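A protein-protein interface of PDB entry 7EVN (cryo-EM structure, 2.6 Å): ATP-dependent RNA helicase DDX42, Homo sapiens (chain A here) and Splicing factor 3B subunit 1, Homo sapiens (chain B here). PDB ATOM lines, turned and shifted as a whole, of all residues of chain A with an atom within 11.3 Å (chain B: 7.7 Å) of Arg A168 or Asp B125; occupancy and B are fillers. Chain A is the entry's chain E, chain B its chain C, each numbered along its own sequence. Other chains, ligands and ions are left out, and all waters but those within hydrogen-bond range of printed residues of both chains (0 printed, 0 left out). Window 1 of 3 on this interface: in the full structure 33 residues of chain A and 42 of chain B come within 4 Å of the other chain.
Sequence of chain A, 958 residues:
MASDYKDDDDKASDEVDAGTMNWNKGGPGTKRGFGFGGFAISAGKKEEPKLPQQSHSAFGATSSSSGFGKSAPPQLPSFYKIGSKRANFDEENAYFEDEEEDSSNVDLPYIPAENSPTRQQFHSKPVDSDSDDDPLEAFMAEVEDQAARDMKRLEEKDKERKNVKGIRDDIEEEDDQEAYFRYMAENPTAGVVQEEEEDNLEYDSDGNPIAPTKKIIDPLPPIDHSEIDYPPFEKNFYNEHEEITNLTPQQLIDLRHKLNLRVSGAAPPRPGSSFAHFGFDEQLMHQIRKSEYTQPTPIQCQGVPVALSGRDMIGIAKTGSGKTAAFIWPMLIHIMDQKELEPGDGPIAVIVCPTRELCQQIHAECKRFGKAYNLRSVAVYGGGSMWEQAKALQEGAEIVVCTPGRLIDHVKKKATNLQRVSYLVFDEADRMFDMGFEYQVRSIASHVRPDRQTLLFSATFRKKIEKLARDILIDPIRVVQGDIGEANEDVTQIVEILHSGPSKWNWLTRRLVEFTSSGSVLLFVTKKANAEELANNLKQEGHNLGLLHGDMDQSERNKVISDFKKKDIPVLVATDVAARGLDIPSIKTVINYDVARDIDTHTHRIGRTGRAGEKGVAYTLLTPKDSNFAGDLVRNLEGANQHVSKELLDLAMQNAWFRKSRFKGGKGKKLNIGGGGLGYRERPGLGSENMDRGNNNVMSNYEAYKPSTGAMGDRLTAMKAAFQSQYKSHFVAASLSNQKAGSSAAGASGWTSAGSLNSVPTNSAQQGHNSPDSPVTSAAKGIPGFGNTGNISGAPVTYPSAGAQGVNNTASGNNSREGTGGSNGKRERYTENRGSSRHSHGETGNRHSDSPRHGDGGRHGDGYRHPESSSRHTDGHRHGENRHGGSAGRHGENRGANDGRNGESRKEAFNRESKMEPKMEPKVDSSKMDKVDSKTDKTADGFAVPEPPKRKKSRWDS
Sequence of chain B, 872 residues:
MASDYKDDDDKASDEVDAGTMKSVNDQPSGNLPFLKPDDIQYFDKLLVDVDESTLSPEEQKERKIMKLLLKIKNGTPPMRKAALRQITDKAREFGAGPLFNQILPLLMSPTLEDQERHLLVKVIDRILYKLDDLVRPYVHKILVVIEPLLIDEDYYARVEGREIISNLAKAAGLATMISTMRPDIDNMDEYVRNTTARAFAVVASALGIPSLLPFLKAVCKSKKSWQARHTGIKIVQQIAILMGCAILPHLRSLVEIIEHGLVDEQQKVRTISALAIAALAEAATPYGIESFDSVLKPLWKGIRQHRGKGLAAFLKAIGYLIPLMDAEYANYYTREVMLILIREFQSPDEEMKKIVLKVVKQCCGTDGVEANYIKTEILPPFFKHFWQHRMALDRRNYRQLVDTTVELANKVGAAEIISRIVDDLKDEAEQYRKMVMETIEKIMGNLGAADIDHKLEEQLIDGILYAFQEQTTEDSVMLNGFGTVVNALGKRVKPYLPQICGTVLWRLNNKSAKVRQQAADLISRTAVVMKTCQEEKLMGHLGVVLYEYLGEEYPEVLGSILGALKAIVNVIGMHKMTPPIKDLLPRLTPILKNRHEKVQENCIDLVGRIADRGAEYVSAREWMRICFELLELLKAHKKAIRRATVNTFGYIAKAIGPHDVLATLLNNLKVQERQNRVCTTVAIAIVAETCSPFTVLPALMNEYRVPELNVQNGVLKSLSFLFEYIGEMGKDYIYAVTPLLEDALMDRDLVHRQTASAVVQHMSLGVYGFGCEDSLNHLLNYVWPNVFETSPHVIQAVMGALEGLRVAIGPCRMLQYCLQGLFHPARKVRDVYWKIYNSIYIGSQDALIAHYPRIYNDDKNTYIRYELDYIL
Of the 19 printed residues of chain B, 4 touch a printed residue of chain A.
Hydrophobic or aromatic side chains of chain B within 4 Å of the printed part of chain A: Tyr B129.
Printed residues of chain A that touch a printed residue of chain B: Ile A167, Arg A168, Ile A171 and Glu A172.
Hydrophobic or aromatic side chains of chain A within 4 Å of the printed part of chain B: Ile A171.
Among the printed residues, 7 pairs touch across the chains.
Among the printed residues, Asp or Glu carboxylates within 4 Å of a Lys or Arg side-chain nitrogen of the other chain: Arg A168 with Asp B125 (3.1 Å) and Glu A172 with Lys B130 (3.5 Å).
Of chain B, only Asp B125 (3.1 Å) and Tyr B129 (3.2 Å) come within 4 Å of Arg A168.
Asp B125 touches just one residue of chain A: Arg A168 (3.1 Å).
No residue of chain A comes within 4 Å of Val B121.
No residue of chain A comes within 4 Å of Ile B124.
No residue of chain A comes within 4 Å of Ile B127.
No residue of chain A comes within 4 Å of Leu B128.
Of chain A, only Ile A167, Arg A168, Ile A171 and Glu A172 come within 4 Å of Tyr B129.
No residue of chain A comes within 4 Å of Asn B167.
Printed residues of chain B within 4 Å of Glu A172: Tyr B129 and Lys B130.
Of the printed residues of chain B, Ile A167 touches Tyr B129.
Printed residues of chain B within 4 Å of Ile A171: Arg B126 and Tyr B129.
Asp A175 touches none of the printed residues of chain B.
Leu B168 touches none of the printed residues of chain A.
The nearest residue of chain B that does not touch Arg A168 is Asn B167 (4.9 Å).
The nearest printed residue of chain B that does not touch Ile A167 is Lys B130 (7.7 Å).
OD1 of Asp B125 lies within salt-bridge range of NH2 of Arg A168, at 3.1 Å.
N of Arg A168 sits at hydrogen-bond distance from OH of Tyr B129, 3.2 Å away.
The side-chain carboxylate of Glu A172 lies within salt-bridge range of the side-chain amino group of Lys B130, at 3.5 Å.
Among the printed residues, merely in contact across the chains: Ile A167 with Tyr B129, Ile A171 with Arg B126, Ile A171 with Tyr B129 and Glu A172 with Tyr B129.
The side-chain carboxylate (OD1) of Asp B125 is in hydrogen-bond range of the side-chain amide nitrogen (ND2) of Asn B167, 3.5 Å away.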
ATOM      1  N   LYS A 165      26.856  20.359 -10.035  1.00  0.00           N
ATOM      2  CA  LYS A 165      27.757  20.934 -11.070  1.00  0.00           C
ATOM      3  C   LYS A 165      27.917  19.932 -12.218  1.00  0.00           C
ATOM      4  O   LYS A 165      28.690  20.218 -13.151  1.00  0.00           O
ATOM      5  CB  LYS A 165      29.125  21.267 -10.466  1.00  0.00           C
ATOM      6  CG  LYS A 165      30.170  21.752 -11.460  1.00  0.00           C
ATOM      7  CD  LYS A 165      31.441  22.238 -10.803  1.00  0.00           C
ATOM      8  CE  LYS A 165      31.242  23.492  -9.979  1.00  0.00           C
ATOM      9  NZ  LYS A 165      30.131  23.344  -9.009  1.00  0.00           N
ATOM     10  N   GLY A 166      27.205  18.805 -12.141  1.00  0.00           N
ATOM     11  CA  GLY A 166      27.287  17.769 -13.188  1.00  0.00           C
ATOM     12  C   GLY A 166      26.771  18.271 -14.524  1.00  0.00           C
ATOM     13  O   GLY A 166      25.756  18.992 -14.530  1.00  0.00           O
ATOM     14  N   ILE A 167      27.452  17.899 -15.610  1.00  0.00           N
ATOM     15  CA  ILE A 167      27.051  18.276 -16.998  1.00  0.00           C
ATOM     16  C   ILE A 167      25.826  17.441 -17.388  1.00  0.00           C
ATOM     17  O   ILE A 167      25.685  16.331 -16.851  1.00  0.00           O
ATOM     18  CB  ILE A 167      28.230  18.027 -17.961  1.00  0.00           C
ATOM     19  CG1 ILE A 167      29.546  18.559 -17.388  1.00  0.00           C
ATOM     20  CG2 ILE A 167      27.943  18.589 -19.345  1.00  0.00           C
ATOM     21  CD1 ILE A 167      30.772  18.086 -18.126  1.00  0.00           C
ATOM     22  N   ARG A 168      24.951  17.979 -18.245  1.00  0.00           N
ATOM     23  CA  ARG A 168      23.766  17.219 -18.726  1.00  0.00           C
ATOM     24  C   ARG A 168      23.973  16.894 -20.209  1.00  0.00           C
ATOM     25  O   ARG A 168      23.882  17.818 -21.034  1.00  0.00           O
ATOM     26  CB  ARG A 168      22.460  17.974 -18.452  1.00  0.00           C
ATOM     27  CG  ARG A 168      22.077  18.016 -16.980  1.00  0.00           C
ATOM     28  CD  ARG A 168      20.681  17.493 -16.698  1.00  0.00           C
ATOM     29  NE  ARG A 168      19.655  18.516 -16.575  1.00  0.00           N
ATOM     30  CZ  ARG A 168      18.524  18.539 -17.271  1.00  0.00           C
ATOM     31  NH1 ARG A 168      18.265  17.587 -18.147  1.00  0.00           N
ATOM     32  NH2 ARG A 168      17.652  19.512 -17.081  1.00  0.00           N
ATOM     33  N   ASP A 169      24.262  15.627 -20.519  1.00  0.00           N
ATOM     34  CA  ASP A 169      24.540  15.186 -21.914  1.00  0.00           C
ATOM     35  C   ASP A 169      23.381  15.533 -22.858  1.00  0.00           C
ATOM     36  O   ASP A 169      23.655  16.045 -23.955  1.00  0.00           O
ATOM     37  CB  ASP A 169      24.819  13.683 -21.952  1.00  0.00           C
ATOM     38  CG  ASP A 169      25.285  13.122 -20.619  1.00  0.00           C
ATOM     39  OD1 ASP A 169      25.229  13.867 -19.616  1.00  0.00           O
ATOM     40  OD2 ASP A 169      25.701  11.945 -20.592  1.00  0.00           O
ATOM     41  N   ASP A 170      22.136  15.303 -22.429  1.00  0.00           N
ATOM     42  CA  ASP A 170      20.950  15.527 -23.302  1.00  0.00           C
ATOM     43  C   ASP A 170      20.800  17.003 -23.694  1.00  0.00           C
ATOM     44  O   ASP A 170      20.554  17.265 -24.885  1.00  0.00           O
ATOM     45  CB  ASP A 170      19.679  14.995 -22.638  1.00  0.00           C
ATOM     46  CG  ASP A 170      19.724  13.498 -22.387  1.00  0.00           C
ATOM     47  OD1 ASP A 170      20.810  12.997 -22.029  1.00  0.00           O
ATOM     48  OD2 ASP A 170      18.679  12.844 -22.557  1.00  0.00           O
ATOM     49  N   ILE A 171      20.959  17.923 -22.739  1.00  0.00           N
ATOM     50  CA  ILE A 171      20.797  19.384 -23.010  1.00  0.00           C
ATOM     51  C   ILE A 171      21.872  19.909 -23.970  1.00  0.00           C
ATOM     52  O   ILE A 171      21.519  20.695 -24.866  1.00  0.00           O
ATOM     53  CB  ILE A 171      20.769  20.193 -21.699  1.00  0.00           C
ATOM     54  CG1 ILE A 171      19.481  19.953 -20.909  1.00  0.00           C
ATOM     55  CG2 ILE A 171      20.980  21.673 -21.981  1.00  0.00           C
ATOM     56  CD1 ILE A 171      19.328  20.857 -19.708  1.00  0.00           C
ATOM     57  N   GLU A 172      23.123  19.473 -23.802  1.00  0.00           N
ATOM     58  CA  GLU A 172      24.254  20.019 -24.608  1.00  0.00           C
ATOM     59  C   GLU A 172      24.530  19.220 -25.887  1.00  0.00           C
ATOM     60  O   GLU A 172      25.436  19.635 -26.633  1.00  0.00           O
ATOM     61  CB  GLU A 172      25.507  20.127 -23.740  1.00  0.00           C
ATOM     62  CG  GLU A 172      25.401  21.222 -22.695  1.00  0.00           C
ATOM     63  CD  GLU A 172      26.636  21.398 -21.830  1.00  0.00           C
ATOM     64  OE1 GLU A 172      27.096  20.397 -21.249  1.00  0.00           O
ATOM     65  OE2 GLU A 172      27.133  22.536 -21.742  1.00  0.00           O
ATOM     66  N   GLU A 173      23.800  18.134 -26.142  1.00  0.00           N
ATOM     67  CA  GLU A 173      24.073  17.332 -27.369  1.00  0.00           C
ATOM     68  C   GLU A 173      22.810  17.216 -28.225  1.00  0.00           C
ATOM     69  O   GLU A 173      21.736  16.925 -27.667  1.00  0.00           O
ATOM     70  CB  GLU A 173      24.689  15.984 -27.000  1.00  0.00           C
ATOM     71  CG  GLU A 173      26.035  16.136 -26.320  1.00  0.00           C
ATOM     72  CD  GLU A 173      26.964  14.945 -26.458  1.00  0.00           C
ATOM     73  OE1 GLU A 173      26.456  13.810 -26.565  1.00  0.00           O
ATOM     74  OE2 GLU A 173      28.193  15.157 -26.461  1.00  0.00           O
ATOM     75  N   GLU A 174      22.966  17.390 -29.542  1.00  0.00           N
ATOM     76  CA  GLU A 174      21.838  17.339 -30.510  1.00  0.00           C
ATOM     77  C   GLU A 174      21.180  15.958 -30.488  1.00  0.00           C
ATOM     78  O   GLU A 174      21.909  14.951 -30.466  1.00  0.00           O
ATOM     79  CB  GLU A 174      22.357  17.607 -31.924  1.00  0.00           C
ATOM     80  CG  GLU A 174      22.433  19.078 -32.281  1.00  0.00           C
ATOM     81  CD  GLU A 174      22.786  19.343 -33.734  1.00  0.00           C
ATOM     82  OE1 GLU A 174      23.152  18.380 -34.437  1.00  0.00           O
ATOM     83  OE2 GLU A 174      22.691  20.511 -34.161  1.00  0.00           O
ATOM     84  N   ASP A 175      19.845  15.909 -30.571  1.00  0.00           N
ATOM     85  CA  ASP A 175      19.095  14.621 -30.577  1.00  0.00           C
ATOM     86  C   ASP A 175      19.082  14.030 -31.993  1.00  0.00           C
ATOM     87  O   ASP A 175      19.512  14.721 -32.933  1.00  0.00           O
ATOM     88  CB  ASP A 175      17.656  14.812 -30.099  1.00  0.00           C
ATOM     89  CG  ASP A 175      17.489  15.952 -29.112  1.00  0.00           C
ATOM     90  OD1 ASP A 175      17.899  15.785 -27.945  1.00  0.00           O
ATOM     91  OD2 ASP A 175      16.954  17.000 -29.523  1.00  0.00           O
ATOM     92  N   THR B  88      18.753  28.479 -25.376  1.00  0.00           N
ATOM     93  CA  THR B  88      19.525  27.859 -24.305  1.00  0.00           C
ATOM     94  C   THR B  88      21.005  28.210 -24.417  1.00  0.00           C
ATOM     95  O   THR B  88      21.736  28.151 -23.425  1.00  0.00           O
ATOM     96  CB  THR B  88      19.319  26.345 -24.286  1.00  0.00           C
ATOM     97  OG1 THR B  88      19.914  25.803 -23.102  1.00  0.00           O
ATOM     98  CG2 THR B  88      19.980  25.699 -25.467  1.00  0.00           C
ATOM     99  N   PHE B 100      12.594  35.939 -17.734  1.00  0.00           N
ATOM    100  CA  PHE B 100      11.402  35.626 -16.958  1.00  0.00           C
ATOM    101  C   PHE B 100      10.360  36.729 -17.046  1.00  0.00           C
ATOM    102  O   PHE B 100       9.159  36.437 -17.013  1.00  0.00           O
ATOM    103  CB  PHE B 100      11.785  35.341 -15.507  1.00  0.00           C
ATOM    104  CG  PHE B 100      12.379  33.980 -15.313  1.00  0.00           C
ATOM    105  CD1 PHE B 100      11.589  32.851 -15.395  1.00  0.00           C
ATOM    106  CD2 PHE B 100      13.730  33.828 -15.087  1.00  0.00           C
ATOM    107  CE1 PHE B 100      12.133  31.603 -15.230  1.00  0.00           C
ATOM    108  CE2 PHE B 100      14.277  32.580 -14.928  1.00  0.00           C
ATOM    109  CZ  PHE B 100      13.477  31.469 -15.000  1.00  0.00           C
ATOM    110  N   LEU B 119       5.564  23.077 -23.427  1.00  0.00           N
ATOM    111  CA  LEU B 119       6.719  23.643 -24.121  1.00  0.00           C
ATOM    112  C   LEU B 119       7.388  24.737 -23.296  1.00  0.00           C
ATOM    113  O   LEU B 119       8.623  24.818 -23.233  1.00  0.00           O
ATOM    114  CB  LEU B 119       6.290  24.194 -25.477  1.00  0.00           C
ATOM    115  CG  LEU B 119       5.848  23.156 -26.503  1.00  0.00           C
ATOM    116  CD1 LEU B 119       5.044  23.802 -27.611  1.00  0.00           C
ATOM    117  CD2 LEU B 119       7.058  22.447 -27.060  1.00  0.00           C
ATOM    118  N   LEU B 120       6.588  25.586 -22.655  1.00  0.00           N
ATOM    119  CA  LEU B 120       7.145  26.632 -21.806  1.00  0.00           C
ATOM    120  C   LEU B 120       7.870  26.038 -20.607  1.00  0.00           C
ATOM    121  O   LEU B 120       8.883  26.578 -20.153  1.00  0.00           O
ATOM    122  CB  LEU B 120       6.035  27.575 -21.350  1.00  0.00           C
ATOM    123  CG  LEU B 120       5.824  28.861 -22.145  1.00  0.00           C
ATOM    124  CD1 LEU B 120       6.917  29.855 -21.828  1.00  0.00           C
ATOM    125  CD2 LEU B 120       5.788  28.581 -23.631  1.00  0.00           C
ATOM    126  N   VAL B 121       7.362  24.924 -20.078  1.00  0.00           N
ATOM    127  CA  VAL B 121       8.042  24.234 -18.985  1.00  0.00           C
ATOM    128  C   VAL B 121       9.404  23.730 -19.444  1.00  0.00           C
ATOM    129  O   VAL B 121      10.400  23.828 -18.715  1.00  0.00           O
ATOM    130  CB  VAL B 121       7.152  23.093 -18.452  1.00  0.00           C
ATOM    131  CG1 VAL B 121       7.937  22.162 -17.558  1.00  0.00           C
ATOM    132  CG2 VAL B 121       5.964  23.656 -17.706  1.00  0.00           C
ATOM    133  N   LYS B 122       9.472  23.186 -20.660  1.00  0.00           N
ATOM    134  CA  LYS B 122      10.764  22.769 -21.202  1.00  0.00           C
ATOM    135  C   LYS B 122      11.726  23.947 -21.324  1.00  0.00           C
ATOM    136  O   LYS B 122      12.913  23.832 -20.988  1.00  0.00           O
ATOM    137  CB  LYS B 122      10.575  22.100 -22.561  1.00  0.00           C
ATOM    138  CG  LYS B 122      10.314  20.617 -22.488  1.00  0.00           C
ATOM    139  CD  LYS B 122       9.548  20.130 -23.704  1.00  0.00           C
ATOM    140  CE  LYS B 122      10.266  20.492 -24.995  1.00  0.00           C
ATOM    141  NZ  LYS B 122      11.490  19.674 -25.203  1.00  0.00           N
ATOM    142  N   VAL B 123      11.230  25.083 -21.819  1.00  0.00           N
ATOM    143  CA  VAL B 123      12.075  26.270 -21.944  1.00  0.00           C
ATOM    144  C   VAL B 123      12.597  26.704 -20.580  1.00  0.00           C
ATOM    145  O   VAL B 123      13.775  27.053 -20.432  1.00  0.00           O
ATOM    146  CB  VAL B 123      11.309  27.409 -22.640  1.00  0.00           C
ATOM    147  CG1 VAL B 123      12.207  28.616 -22.799  1.00  0.00           C
ATOM    148  CG2 VAL B 123      10.800  26.966 -23.990  1.00  0.00           C
ATOM    149  N   ILE B 124      11.723  26.713 -19.570  1.00  0.00           N
ATOM    150  CA  ILE B 124      12.125  27.156 -18.237  1.00  0.00           C
ATOM    151  C   ILE B 124      13.189  26.229 -17.671  1.00  0.00           C
ATOM    152  O   ILE B 124      14.161  26.677 -17.055  1.00  0.00           O
ATOM    153  CB  ILE B 124      10.907  27.244 -17.303  1.00  0.00           C
ATOM    154  CG1 ILE B 124      10.035  28.439 -17.666  1.00  0.00           C
ATOM    155  CG2 ILE B 124      11.348  27.364 -15.864  1.00  0.00           C
ATOM    156  CD1 ILE B 124       8.581  28.222 -17.389  1.00  0.00           C
ATOM    157  N   ASP B 125      13.021  24.923 -17.874  1.00  0.00           N
ATOM    158  CA  ASP B 125      14.041  23.972 -17.446  1.00  0.00           C
ATOM    159  C   ASP B 125      15.387  24.287 -18.090  1.00  0.00           C
ATOM    160  O   ASP B 125      16.417  24.376 -17.407  1.00  0.00           O
ATOM    161  CB  ASP B 125      13.589  22.552 -17.784  1.00  0.00           C
ATOM    162  CG  ASP B 125      14.649  21.504 -17.493  1.00  0.00           C
ATOM    163  OD1 ASP B 125      15.610  21.785 -16.748  1.00  0.00           O
ATOM    164  OD2 ASP B 125      14.518  20.381 -18.021  1.00  0.00           O
ATOM    165  N   ARG B 126      15.397  24.464 -19.413  1.00  0.00           N
ATOM    166  CA  ARG B 126      16.670  24.659 -20.099  1.00  0.00           C
ATOM    167  C   ARG B 126      17.335  25.974 -19.712  1.00  0.00           C
ATOM    168  O   ARG B 126      18.565  26.040 -19.648  1.00  0.00           O
ATOM    169  CB  ARG B 126      16.479  24.574 -21.610  1.00  0.00           C
ATOM    170  CG  ARG B 126      16.118  23.184 -22.069  1.00  0.00           C
ATOM    171  CD  ARG B 126      15.616  23.172 -23.489  1.00  0.00           C
ATOM    172  NE  ARG B 126      16.716  23.137 -24.443  1.00  0.00           N
ATOM    173  CZ  ARG B 126      17.212  22.024 -24.971  1.00  0.00           C
ATOM    174  NH1 ARG B 126      16.705  20.847 -24.640  1.00  0.00           N
ATOM    175  NH2 ARG B 126      18.217  22.092 -25.831  1.00  0.00           N
ATOM    176  N   ILE B 127      16.560  27.027 -19.451  1.00  0.00           N
ATOM    177  CA  ILE B 127      17.198  28.279 -19.056  1.00  0.00           C
ATOM    178  C   ILE B 127      17.630  28.268 -17.594  1.00  0.00           C
ATOM    179  O   ILE B 127      18.644  28.888 -17.257  1.00  0.00           O
ATOM    180  CB  ILE B 127      16.302  29.501 -19.327  1.00  0.00           C
ATOM    181  CG1 ILE B 127      15.042  29.467 -18.467  1.00  0.00           C
ATOM    182  CG2 ILE B 127      15.953  29.589 -20.800  1.00  0.00           C
ATOM    183  CD1 ILE B 127      14.262  30.742 -18.498  1.00  0.00           C
ATOM    184  N   LEU B 128      16.900  27.578 -16.716  1.00  0.00           N
ATOM    185  CA  LEU B 128      17.324  27.411 -15.333  1.00  0.00           C
ATOM    186  C   LEU B 128      18.586  26.577 -15.216  1.00  0.00           C
ATOM    187  O   LEU B 128      19.337  26.742 -14.253  1.00  0.00           O
ATOM    188  CB  LEU B 128      16.208  26.755 -14.519  1.00  0.00           C
ATOM    189  CG  LEU B 128      15.519  27.576 -13.435  1.00  0.00           C
ATOM    190  CD1 LEU B 128      15.540  29.035 -13.795  1.00  0.00           C
ATOM    191  CD2 LEU B 128      14.097  27.096 -13.234  1.00  0.00           C
ATOM    192  N   TYR B 129      18.828  25.678 -16.170  1.00  0.00           N
ATOM    193  CA  TYR B 129      20.076  24.924 -16.156  1.00  0.00           C
ATOM    194  C   TYR B 129      21.281  25.828 -16.395  1.00  0.00           C
ATOM    195  O   TYR B 129      22.353  25.607 -15.824  1.00  0.00           O
ATOM    196  CB  TYR B 129      20.028  23.820 -17.203  1.00  0.00           C
ATOM    197  CG  TYR B 129      21.347  23.133 -17.424  1.00  0.00           C
ATOM    198  CD1 TYR B 129      22.027  23.265 -18.622  1.00  0.00           C
ATOM    199  CD2 TYR B 129      21.908  22.343 -16.438  1.00  0.00           C
ATOM    200  CE1 TYR B 129      23.229  22.630 -18.827  1.00  0.00           C
ATOM    201  CE2 TYR B 129      23.108  21.705 -16.636  1.00  0.00           C
ATOM    202  CZ  TYR B 129      23.765  21.853 -17.828  1.00  0.00           C
ATOM    203  OH  TYR B 129      24.964  21.215 -18.024  1.00  0.00           O
ATOM    204  N   LYS B 130      21.128  26.846 -17.243  1.00  0.00           N
ATOM    205  CA  LYS B 130      22.222  27.754 -17.580  1.00  0.00           C
ATOM    206  C   LYS B 130      22.379  28.855 -16.537  1.00  0.00           C
ATOM    207  O   LYS B 130      23.476  29.076 -16.020  1.00  0.00           O
ATOM    208  CB  LYS B 130      21.996  28.365 -18.965  1.00  0.00           C
ATOM    209  CG  LYS B 130      22.089  27.371 -20.089  1.00  0.00           C
ATOM    210  CD  LYS B 130      23.492  26.841 -20.218  1.00  0.00           C
ATOM    211  CE  LYS B 130      23.636  25.977 -21.446  1.00  0.00           C
ATOM    212  NZ  LYS B 130      24.969  25.330 -21.489  1.00  0.00           N
ATOM    213  N   LEU B 131      21.297  29.566 -16.241  1.00  0.00           N
ATOM    214  CA  LEU B 131      21.289  30.505 -15.129  1.00  0.00           C
ATOM    215  C   LEU B 131      21.141  29.738 -13.829  1.00  0.00           C
ATOM    216  O   LEU B 131      20.025  29.352 -13.474  1.00  0.00           O
ATOM    217  CB  LEU B 131      20.135  31.496 -15.255  1.00  0.00           C
ATOM    218  CG  LEU B 131      19.748  32.023 -16.627  1.00  0.00           C
ATOM    219  CD1 LEU B 131      18.578  32.954 -16.475  1.00  0.00           C
ATOM    220  CD2 LEU B 131      20.917  32.748 -17.236  1.00  0.00           C
ATOM    221  N   GLU B 163       7.419  20.386 -11.532  1.00  0.00           N
ATOM    222  CA  GLU B 163       8.688  20.427 -12.260  1.00  0.00           C
ATOM    223  C   GLU B 163       9.342  21.801 -12.176  1.00  0.00           C
ATOM    224  O   GLU B 163      10.561  21.903 -11.979  1.00  0.00           O
ATOM    225  CB  GLU B 163       8.489  20.028 -13.719  1.00  0.00           C
ATOM    226  CG  GLU B 163       7.609  18.823 -13.899  1.00  0.00           C
ATOM    227  CD  GLU B 163       7.840  18.101 -15.208  1.00  0.00           C
ATOM    228  OE1 GLU B 163       8.424  16.999 -15.177  1.00  0.00           O
ATOM    229  OE2 GLU B 163       7.413  18.623 -16.259  1.00  0.00           O
ATOM    230  N   ILE B 164       8.559  22.867 -12.327  1.00  0.00           N
ATOM    231  CA  ILE B 164       9.147  24.201 -12.282  1.00  0.00           C
ATOM    232  C   ILE B 164       9.705  24.493 -10.893  1.00  0.00           C
ATOM    233  O   ILE B 164      10.811  25.031 -10.752  1.00  0.00           O
ATOM    234  CB  ILE B 164       8.128  25.266 -12.718  1.00  0.00           C
ATOM    235  CG1 ILE B 164       7.598  24.957 -14.113  1.00  0.00           C
ATOM    236  CG2 ILE B 164       8.777  26.630 -12.727  1.00  0.00           C
ATOM    237  CD1 ILE B 164       6.760  26.060 -14.692  1.00  0.00           C
ATOM    238  N   ASN B 167      13.038  22.504 -10.439  1.00  0.00           N
ATOM    239  CA  ASN B 167      14.177  23.085 -11.140  1.00  0.00           C
ATOM    240  C   ASN B 167      14.613  24.390 -10.493  1.00  0.00           C
ATOM    241  O   ASN B 167      15.810  24.683 -10.414  1.00  0.00           O
ATOM    242  CB  ASN B 167      13.837  23.303 -12.613  1.00  0.00           C
ATOM    243  CG  ASN B 167      13.832  22.019 -13.402  1.00  0.00           C
ATOM    244  OD1 ASN B 167      12.835  21.663 -14.016  1.00  0.00           O
ATOM    245  ND2 ASN B 167      14.951  21.316 -13.393  1.00  0.00           N
ATOM    246  N   LEU B 168      13.656  25.180 -10.006  1.00  0.00           N
ATOM    247  CA  LEU B 168      14.002  26.426  -9.339  1.00  0.00           C
ATOM    248  C   LEU B 168      14.721  26.173  -8.021  1.00  0.00           C
ATOM    249  O   LEU B 168      15.688  26.870  -7.692  1.00  0.00           O
ATOM    250  CB  LEU B 168      12.741  27.251  -9.113  1.00  0.00           C
ATOM    251  CG  LEU B 168      12.900  28.592  -8.412  1.00  0.00           C
ATOM    252  CD1 LEU B 168      13.751  29.514  -9.248  1.00  0.00           C
ATOM    253  CD2 LEU B 168      11.541  29.195  -8.171  1.00  0.00           C
